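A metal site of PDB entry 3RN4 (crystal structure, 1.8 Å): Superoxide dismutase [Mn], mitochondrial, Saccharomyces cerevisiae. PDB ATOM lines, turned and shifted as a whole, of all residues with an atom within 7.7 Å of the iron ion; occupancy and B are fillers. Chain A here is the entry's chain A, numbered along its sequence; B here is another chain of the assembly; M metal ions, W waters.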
ATOM      1  N   HIS A  34      -8.572  12.283 -23.131  1.00  0.00           N
ATOM      2  CA  HIS A  34      -9.648  12.987 -23.827  1.00  0.00           C
ATOM      3  C   HIS A  34      -9.285  13.198 -25.301  1.00  0.00           C
ATOM      4  O   HIS A  34     -10.112  13.001 -26.190  1.00  0.00           O
ATOM      5  CB  HIS A  34      -9.902  14.328 -23.115  1.00  0.00           C
ATOM      6  CG  HIS A  34     -11.297  14.855 -23.285  1.00  0.00           C
ATOM      7  ND1 HIS A  34     -11.710  16.031 -22.689  1.00  0.00           N
ATOM      8  CD2 HIS A  34     -12.368  14.371 -23.957  1.00  0.00           C
ATOM      9  CE1 HIS A  34     -12.982  16.246 -22.992  1.00  0.00           C
ATOM     10  NE2 HIS A  34     -13.407  15.251 -23.757  1.00  0.00           N
ATOM     11  N   TYR A  35      -8.024  13.570 -25.547  1.00  0.00           N
ATOM     12  CA  TYR A  35      -7.534  13.829 -26.924  1.00  0.00           C
ATOM     13  C   TYR A  35      -7.138  12.556 -27.674  1.00  0.00           C
ATOM     14  O   TYR A  35      -7.674  12.262 -28.755  1.00  0.00           O
ATOM     15  CB  TYR A  35      -6.367  14.821 -26.825  1.00  0.00           C
ATOM     16  CG  TYR A  35      -5.672  15.177 -28.123  1.00  0.00           C
ATOM     17  CD1 TYR A  35      -6.215  16.119 -29.000  1.00  0.00           C
ATOM     18  CD2 TYR A  35      -4.444  14.603 -28.446  1.00  0.00           C
ATOM     19  CE1 TYR A  35      -5.580  16.453 -30.168  1.00  0.00           C
ATOM     20  CE2 TYR A  35      -3.795  14.935 -29.618  1.00  0.00           C
ATOM     21  CZ  TYR A  35      -4.359  15.870 -30.483  1.00  0.00           C
ATOM     22  OH  TYR A  35      -3.712  16.192 -31.655  1.00  0.00           O
ATOM     23  N   HIS A  38     -10.551   9.541 -26.642  1.00  0.00           N
ATOM     24  CA  HIS A  38     -11.926   9.944 -26.919  1.00  0.00           C
ATOM     25  C   HIS A  38     -12.040  10.668 -28.244  1.00  0.00           C
ATOM     26  O   HIS A  38     -12.832  10.272 -29.095  1.00  0.00           O
ATOM     27  CB  HIS A  38     -12.510  10.778 -25.775  1.00  0.00           C
ATOM     28  CG  HIS A  38     -12.617  10.020 -24.486  1.00  0.00           C
ATOM     29  ND1 HIS A  38     -13.660   9.155 -24.230  1.00  0.00           N
ATOM     30  CD2 HIS A  38     -11.796   9.942 -23.412  1.00  0.00           C
ATOM     31  CE1 HIS A  38     -13.476   8.584 -23.051  1.00  0.00           C
ATOM     32  NE2 HIS A  38     -12.365   9.042 -22.529  1.00  0.00           N
ATOM     33  N   HIS A  39     -11.266  11.728 -28.433  1.00  0.00           N
ATOM     34  CA  HIS A  39     -11.413  12.487 -29.676  1.00  0.00           C
ATOM     35  C   HIS A  39     -11.070  11.624 -30.880  1.00  0.00           C
ATOM     36  O   HIS A  39     -11.754  11.668 -31.916  1.00  0.00           O
ATOM     37  CB  HIS A  39     -10.567  13.756 -29.653  1.00  0.00           C
ATOM     38  CG  HIS A  39     -11.036  14.798 -30.623  1.00  0.00           C
ATOM     39  ND1 HIS A  39     -10.507  16.069 -30.662  1.00  0.00           N
ATOM     40  CD2 HIS A  39     -11.995  14.756 -31.582  1.00  0.00           C
ATOM     41  CE1 HIS A  39     -11.121  16.770 -31.607  1.00  0.00           C
ATOM     42  NE2 HIS A  39     -12.030  15.995 -32.180  1.00  0.00           N
ATOM     43  N   TYR A  42     -13.867   9.466 -32.092  1.00  0.00           N
ATOM     44  CA  TYR A  42     -14.885  10.181 -32.860  1.00  0.00           C
ATOM     45  C   TYR A  42     -14.366  10.457 -34.280  1.00  0.00           C
ATOM     46  O   TYR A  42     -15.102  10.357 -35.252  1.00  0.00           O
ATOM     47  CB  TYR A  42     -15.289  11.487 -32.164  1.00  0.00           C
ATOM     48  CG  TYR A  42     -15.949  11.265 -30.809  1.00  0.00           C
ATOM     49  CD1 TYR A  42     -17.064  10.425 -30.681  1.00  0.00           C
ATOM     50  CD2 TYR A  42     -15.480  11.914 -29.672  1.00  0.00           C
ATOM     51  CE1 TYR A  42     -17.663  10.205 -29.442  1.00  0.00           C
ATOM     52  CE2 TYR A  42     -16.075  11.704 -28.420  1.00  0.00           C
ATOM     53  CZ  TYR A  42     -17.166  10.849 -28.334  1.00  0.00           C
ATOM     54  OH  TYR A  42     -17.752  10.658 -27.090  1.00  0.00           O
ATOM     55  N   GLY A  85     -19.028  14.458 -32.179  1.00  0.00           N
ATOM     56  CA  GLY A  85     -17.893  14.299 -31.272  1.00  0.00           C
ATOM     57  C   GLY A  85     -16.643  14.931 -31.852  1.00  0.00           C
ATOM     58  O   GLY A  85     -15.843  15.530 -31.131  1.00  0.00           O
ATOM     59  N   ASN A  88     -17.286  18.939 -31.783  1.00  0.00           N
ATOM     60  CA  ASN A  88     -17.357  19.513 -30.448  1.00  0.00           C
ATOM     61  C   ASN A  88     -16.021  19.567 -29.767  1.00  0.00           C
ATOM     62  O   ASN A  88     -15.687  20.558 -29.126  1.00  0.00           O
ATOM     63  CB  ASN A  88     -18.371  18.727 -29.561  1.00  0.00           C
ATOM     64  CG  ASN A  88     -19.797  19.039 -29.896  1.00  0.00           C
ATOM     65  OD1 ASN A  88     -20.097  20.049 -30.551  1.00  0.00           O
ATOM     66  ND2 ASN A  88     -20.713  18.151 -29.467  1.00  0.00           N
ATOM     67  N   HIS A  89     -15.230  18.495 -29.888  1.00  0.00           N
ATOM     68  CA  HIS A  89     -13.940  18.526 -29.197  1.00  0.00           C
ATOM     69  C   HIS A  89     -12.970  19.489 -29.904  1.00  0.00           C
ATOM     70  O   HIS A  89     -12.110  20.089 -29.263  1.00  0.00           O
ATOM     71  CB  HIS A  89     -13.367  17.122 -29.057  1.00  0.00           C
ATOM     72  CG  HIS A  89     -14.157  16.268 -28.112  1.00  0.00           C
ATOM     73  ND1 HIS A  89     -15.271  15.555 -28.508  1.00  0.00           N
ATOM     74  CD2 HIS A  89     -14.008  16.025 -26.784  1.00  0.00           C
ATOM     75  CE1 HIS A  89     -15.782  14.918 -27.472  1.00  0.00           C
ATOM     76  NE2 HIS A  89     -15.039  15.188 -26.406  1.00  0.00           N
ATOM     77  N   PHE A  92     -13.832  22.676 -28.419  1.00  0.00           N
ATOM     78  CA  PHE A  92     -13.387  22.646 -27.050  1.00  0.00           C
ATOM     79  C   PHE A  92     -11.903  23.027 -26.905  1.00  0.00           C
ATOM     80  O   PHE A  92     -11.570  23.926 -26.152  1.00  0.00           O
ATOM     81  CB  PHE A  92     -13.678  21.238 -26.434  1.00  0.00           C
ATOM     82  CG  PHE A  92     -13.528  21.144 -24.932  1.00  0.00           C
ATOM     83  CD1 PHE A  92     -14.208  21.997 -24.070  1.00  0.00           C
ATOM     84  CD2 PHE A  92     -12.733  20.134 -24.366  1.00  0.00           C
ATOM     85  CE1 PHE A  92     -14.080  21.888 -22.708  1.00  0.00           C
ATOM     86  CE2 PHE A  92     -12.628  20.009 -22.992  1.00  0.00           C
ATOM     87  CZ  PHE A  92     -13.293  20.859 -22.156  1.00  0.00           C
ATOM     88  N   TRP A  93     -10.995  22.338 -27.609  1.00  0.00           N
ATOM     89  CA  TRP A  93      -9.580  22.627 -27.357  1.00  0.00           C
ATOM     90  C   TRP A  93      -9.259  24.059 -27.746  1.00  0.00           C
ATOM     91  O   TRP A  93      -8.441  24.706 -27.100  1.00  0.00           O
ATOM     92  CB  TRP A  93      -8.653  21.703 -28.158  1.00  0.00           C
ATOM     93  CG  TRP A  93      -9.005  20.240 -28.113  1.00  0.00           C
ATOM     94  CD1 TRP A  93      -9.172  19.419 -29.171  1.00  0.00           C
ATOM     95  CD2 TRP A  93      -9.195  19.447 -26.929  1.00  0.00           C
ATOM     96  NE1 TRP A  93      -9.472  18.135 -28.736  1.00  0.00           N
ATOM     97  CE2 TRP A  93      -9.487  18.132 -27.364  1.00  0.00           C
ATOM     98  CE3 TRP A  93      -9.152  19.707 -25.557  1.00  0.00           C
ATOM     99  CZ2 TRP A  93      -9.746  17.079 -26.468  1.00  0.00           C
ATOM    100  CZ3 TRP A  93      -9.389  18.651 -24.660  1.00  0.00           C
ATOM    101  CH2 TRP A  93      -9.700  17.370 -25.132  1.00  0.00           C
ATOM    102  N   GLY A 140     -23.307  15.411 -22.058  1.00  0.00           N
ATOM    103  CA  GLY A 140     -23.624  16.468 -23.020  1.00  0.00           C
ATOM    104  C   GLY A 140     -22.702  17.652 -22.873  1.00  0.00           C
ATOM    105  O   GLY A 140     -21.613  17.526 -22.325  1.00  0.00           O
ATOM    106  N   TRP A 141     -23.190  18.803 -23.338  1.00  0.00           N
ATOM    107  CA  TRP A 141     -22.376  20.018 -23.528  1.00  0.00           C
ATOM    108  C   TRP A 141     -23.198  21.234 -23.123  1.00  0.00           C
ATOM    109  O   TRP A 141     -24.432  21.206 -23.172  1.00  0.00           O
ATOM    110  CB  TRP A 141     -22.014  20.189 -25.011  1.00  0.00           C
ATOM    111  CG  TRP A 141     -21.070  19.167 -25.501  1.00  0.00           C
ATOM    112  CD1 TRP A 141     -21.381  17.874 -25.879  1.00  0.00           C
ATOM    113  CD2 TRP A 141     -19.647  19.297 -25.616  1.00  0.00           C
ATOM    114  NE1 TRP A 141     -20.209  17.208 -26.215  1.00  0.00           N
ATOM    115  CE2 TRP A 141     -19.146  18.054 -26.084  1.00  0.00           C
ATOM    116  CE3 TRP A 141     -18.740  20.340 -25.408  1.00  0.00           C
ATOM    117  CZ2 TRP A 141     -17.788  17.821 -26.311  1.00  0.00           C
ATOM    118  CZ3 TRP A 141     -17.385  20.119 -25.627  1.00  0.00           C
ATOM    119  CH2 TRP A 141     -16.921  18.851 -26.080  1.00  0.00           C
ATOM    120  N   ASN A 161     -25.351  14.227 -25.336  1.00  0.00           N
ATOM    121  CA  ASN A 161     -24.505  13.285 -26.067  1.00  0.00           C
ATOM    122  C   ASN A 161     -23.496  14.061 -26.909  1.00  0.00           C
ATOM    123  O   ASN A 161     -22.798  14.891 -26.363  1.00  0.00           O
ATOM    124  CB  ASN A 161     -25.407  12.318 -26.840  1.00  0.00           C
ATOM    125  CG  ASN A 161     -26.421  11.644 -25.904  1.00  0.00           C
ATOM    126  OD1 ASN A 161     -27.620  11.562 -26.197  1.00  0.00           O
ATOM    127  ND2 ASN A 161     -25.940  11.257 -24.751  1.00  0.00           N
ATOM    128  N   GLN A 162     -23.404  13.797 -28.211  1.00  0.00           N
ATOM    129  CA  GLN A 162     -22.551  14.670 -29.062  1.00  0.00           C
ATOM    130  C   GLN A 162     -23.379  15.507 -30.007  1.00  0.00           C
ATOM    131  O   GLN A 162     -22.920  15.921 -31.078  1.00  0.00           O
ATOM    132  CB  GLN A 162     -21.484  13.874 -29.860  1.00  0.00           C
ATOM    133  CG  GLN A 162     -20.432  13.152 -28.977  1.00  0.00           C
ATOM    134  CD  GLN A 162     -19.645  14.065 -28.070  1.00  0.00           C
ATOM    135  OE1 GLN A 162     -19.638  15.282 -28.242  1.00  0.00           O
ATOM    136  NE2 GLN A 162     -18.954  13.473 -27.123  1.00  0.00           N
ATOM    137  N   ASP A 176     -17.441  20.857 -22.169  1.00  0.00           N
ATOM    138  CA  ASP A 176     -17.779  19.423 -22.176  1.00  0.00           C
ATOM    139  C   ASP A 176     -18.270  19.022 -20.798  1.00  0.00           C
ATOM    140  O   ASP A 176     -17.585  19.231 -19.808  1.00  0.00           O
ATOM    141  CB  ASP A 176     -16.499  18.638 -22.566  1.00  0.00           C
ATOM    142  CG  ASP A 176     -16.754  17.204 -22.922  1.00  0.00           C
ATOM    143  OD1 ASP A 176     -15.777  16.541 -23.364  1.00  0.00           O
ATOM    144  OD2 ASP A 176     -17.914  16.736 -22.770  1.00  0.00           O
ATOM    145  N   ALA A 177     -19.462  18.418 -20.748  1.00  0.00           N
ATOM    146  CA  ALA A 177     -20.033  17.940 -19.493  1.00  0.00           C
ATOM    147  C   ALA A 177     -20.071  16.414 -19.417  1.00  0.00           C
ATOM    148  O   ALA A 177     -20.600  15.852 -18.446  1.00  0.00           O
ATOM    149  CB  ALA A 177     -21.466  18.509 -19.281  1.00  0.00           C
ATOM    150  N   TRP A 178     -19.490  15.722 -20.400  1.00  0.00           N
ATOM    151  CA  TRP A 178     -19.377  14.262 -20.262  1.00  0.00           C
ATOM    152  C   TRP A 178     -18.530  13.945 -19.047  1.00  0.00           C
ATOM    153  O   TRP A 178     -17.569  14.654 -18.731  1.00  0.00           O
ATOM    154  CB  TRP A 178     -18.707  13.628 -21.489  1.00  0.00           C
ATOM    155  CG  TRP A 178     -19.588  13.484 -22.661  1.00  0.00           C
ATOM    156  CD1 TRP A 178     -20.270  14.467 -23.321  1.00  0.00           C
ATOM    157  CD2 TRP A 178     -19.862  12.260 -23.350  1.00  0.00           C
ATOM    158  NE1 TRP A 178     -20.957  13.924 -24.400  1.00  0.00           N
ATOM    159  CE2 TRP A 178     -20.715  12.577 -24.440  1.00  0.00           C
ATOM    160  CE3 TRP A 178     -19.450  10.923 -23.161  1.00  0.00           C
ATOM    161  CZ2 TRP A 178     -21.198  11.583 -25.322  1.00  0.00           C
ATOM    162  CZ3 TRP A 178     -19.935   9.949 -24.034  1.00  0.00           C
ATOM    163  CH2 TRP A 178     -20.793  10.276 -25.093  1.00  0.00           C
ATOM    164  N   GLU A 179     -18.829  12.841 -18.370  1.00  0.00           N
ATOM    165  CA  GLU A 179     -18.021  12.511 -17.211  1.00  0.00           C
ATOM    166  C   GLU A 179     -16.529  12.338 -17.505  1.00  0.00           C
ATOM    167  O   GLU A 179     -15.685  12.715 -16.668  1.00  0.00           O
ATOM    168  CB  GLU A 179     -18.622  11.314 -16.438  1.00  0.00           C
ATOM    169  CG  GLU A 179     -20.047  11.645 -15.920  1.00  0.00           C
ATOM    170  CD  GLU A 179     -20.670  10.462 -15.184  1.00  0.00           C
ATOM    171  OE1 GLU A 179     -20.636   9.348 -15.745  1.00  0.00           O
ATOM    172  OE2 GLU A 179     -21.156  10.630 -14.040  1.00  0.00           O
ATOM    173  N   HIS A 180     -16.162  11.815 -18.689  1.00  0.00           N
ATOM    174  CA  HIS A 180     -14.734  11.653 -19.010  1.00  0.00           C
ATOM    175  C   HIS A 180     -13.976  12.977 -19.021  1.00  0.00           C
ATOM    176  O   HIS A 180     -12.751  13.007 -18.978  1.00  0.00           O
ATOM    177  CB  HIS A 180     -14.539  10.897 -20.348  1.00  0.00           C
ATOM    178  CG  HIS A 180     -15.005  11.647 -21.559  1.00  0.00           C
ATOM    179  ND1 HIS A 180     -16.007  11.174 -22.377  1.00  0.00           N
ATOM    180  CD2 HIS A 180     -14.614  12.826 -22.094  1.00  0.00           C
ATOM    181  CE1 HIS A 180     -16.197  12.019 -23.373  1.00  0.00           C
ATOM    182  NE2 HIS A 180     -15.372  13.026 -23.235  1.00  0.00           N
ATOM    183  N   ALA A 181     -14.700  14.091 -19.016  1.00  0.00           N
ATOM    184  CA  ALA A 181     -14.058  15.404 -19.073  1.00  0.00           C
ATOM    185  C   ALA A 181     -13.518  15.805 -17.718  1.00  0.00           C
ATOM    186  O   ALA A 181     -12.705  16.714 -17.626  1.00  0.00           O
ATOM    187  CB  ALA A 181     -15.056  16.488 -19.616  1.00  0.00           C
ATOM    188  N   TYR A 193     -15.594  21.140 -11.174  1.00  0.00           N
ATOM    189  CA  TYR A 193     -15.041  21.206 -12.497  1.00  0.00           C
ATOM    190  C   TYR A 193     -15.632  22.377 -13.270  1.00  0.00           C
ATOM    191  O   TYR A 193     -14.891  23.144 -13.910  1.00  0.00           O
ATOM    192  CB  TYR A 193     -15.312  19.881 -13.257  1.00  0.00           C
ATOM    193  CG  TYR A 193     -15.202  19.952 -14.765  1.00  0.00           C
ATOM    194  CD1 TYR A 193     -13.971  20.141 -15.399  1.00  0.00           C
ATOM    195  CD2 TYR A 193     -16.315  19.720 -15.566  1.00  0.00           C
ATOM    196  CE1 TYR A 193     -13.885  20.173 -16.801  1.00  0.00           C
ATOM    197  CE2 TYR A 193     -16.241  19.745 -16.951  1.00  0.00           C
ATOM    198  CZ  TYR A 193     -15.011  19.964 -17.576  1.00  0.00           C
ATOM    199  OH  TYR A 193     -14.945  19.969 -18.953  1.00  0.00           O
ATOM    200  N   GLU B 179     -20.302   6.589 -17.736  1.00  0.00           N
ATOM    201  CA  GLU B 179     -18.869   6.532 -17.513  1.00  0.00           C
ATOM    202  C   GLU B 179     -18.458   6.375 -16.047  1.00  0.00           C
ATOM    203  O   GLU B 179     -17.466   5.680 -15.753  1.00  0.00           O
ATOM    204  CB  GLU B 179     -18.151   7.709 -18.214  1.00  0.00           C
ATOM    205  CG  GLU B 179     -18.376   7.663 -19.750  1.00  0.00           C
ATOM    206  CD  GLU B 179     -17.703   8.837 -20.454  1.00  0.00           C
ATOM    207  OE1 GLU B 179     -17.906   9.980 -19.997  1.00  0.00           O
ATOM    208  OE2 GLU B 179     -16.948   8.622 -21.432  1.00  0.00           O
HETATM  209 FE    FE M   1     -15.451  14.876 -24.321  1.00  0.00          FE
HETATM  210  O   HOH W   1     -17.507  14.594 -24.783  1.00  0.00           O
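The side-chain carboxylate (OD2) of Asp 176 lies within hydrogen-bond range of the backbone NH (N) of Trp 178, 3.0 Å away. O of Asp 176 sits at hydrogen-bond distance from OH of Tyr 193, at 2.9 Å. The backbone carbonyl oxygen of His 89 lies close to the indole nitrogen of Trp 93 (3.3 Å). ND1 of His 89 is in hydrogen-bond range of O of Gly 85 (2.7 Å). The backbone NH (N) of His 180 sits at hydrogen-bond distance from the side-chain carboxylate (OE1) of Glu 179 of chain B, 2.8 Å away. The backbone carbonyl oxygen (O) of His 34 lies within hydrogen-bond range of the backbone NH (N) of His 39, 2.8 Å away.
Water W1 lies within hydrogen-bond range of OD2 of Asp 176 and NE2 of Gln 162.
The nearest printed residue that does not touch the iron ion is Trp 141 (4.3 Å).
OD1 of Asp 176 is bound to the iron ion, at 1.9 Å. Water W1 is bound to the iron ion, at 2.1 Å. The iron ion is bound by NE2 of His 89. A ring nitrogen (NE2) of His 180 binds the iron ion. NE2 of His 34 binds the iron ion (2.2 Å).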
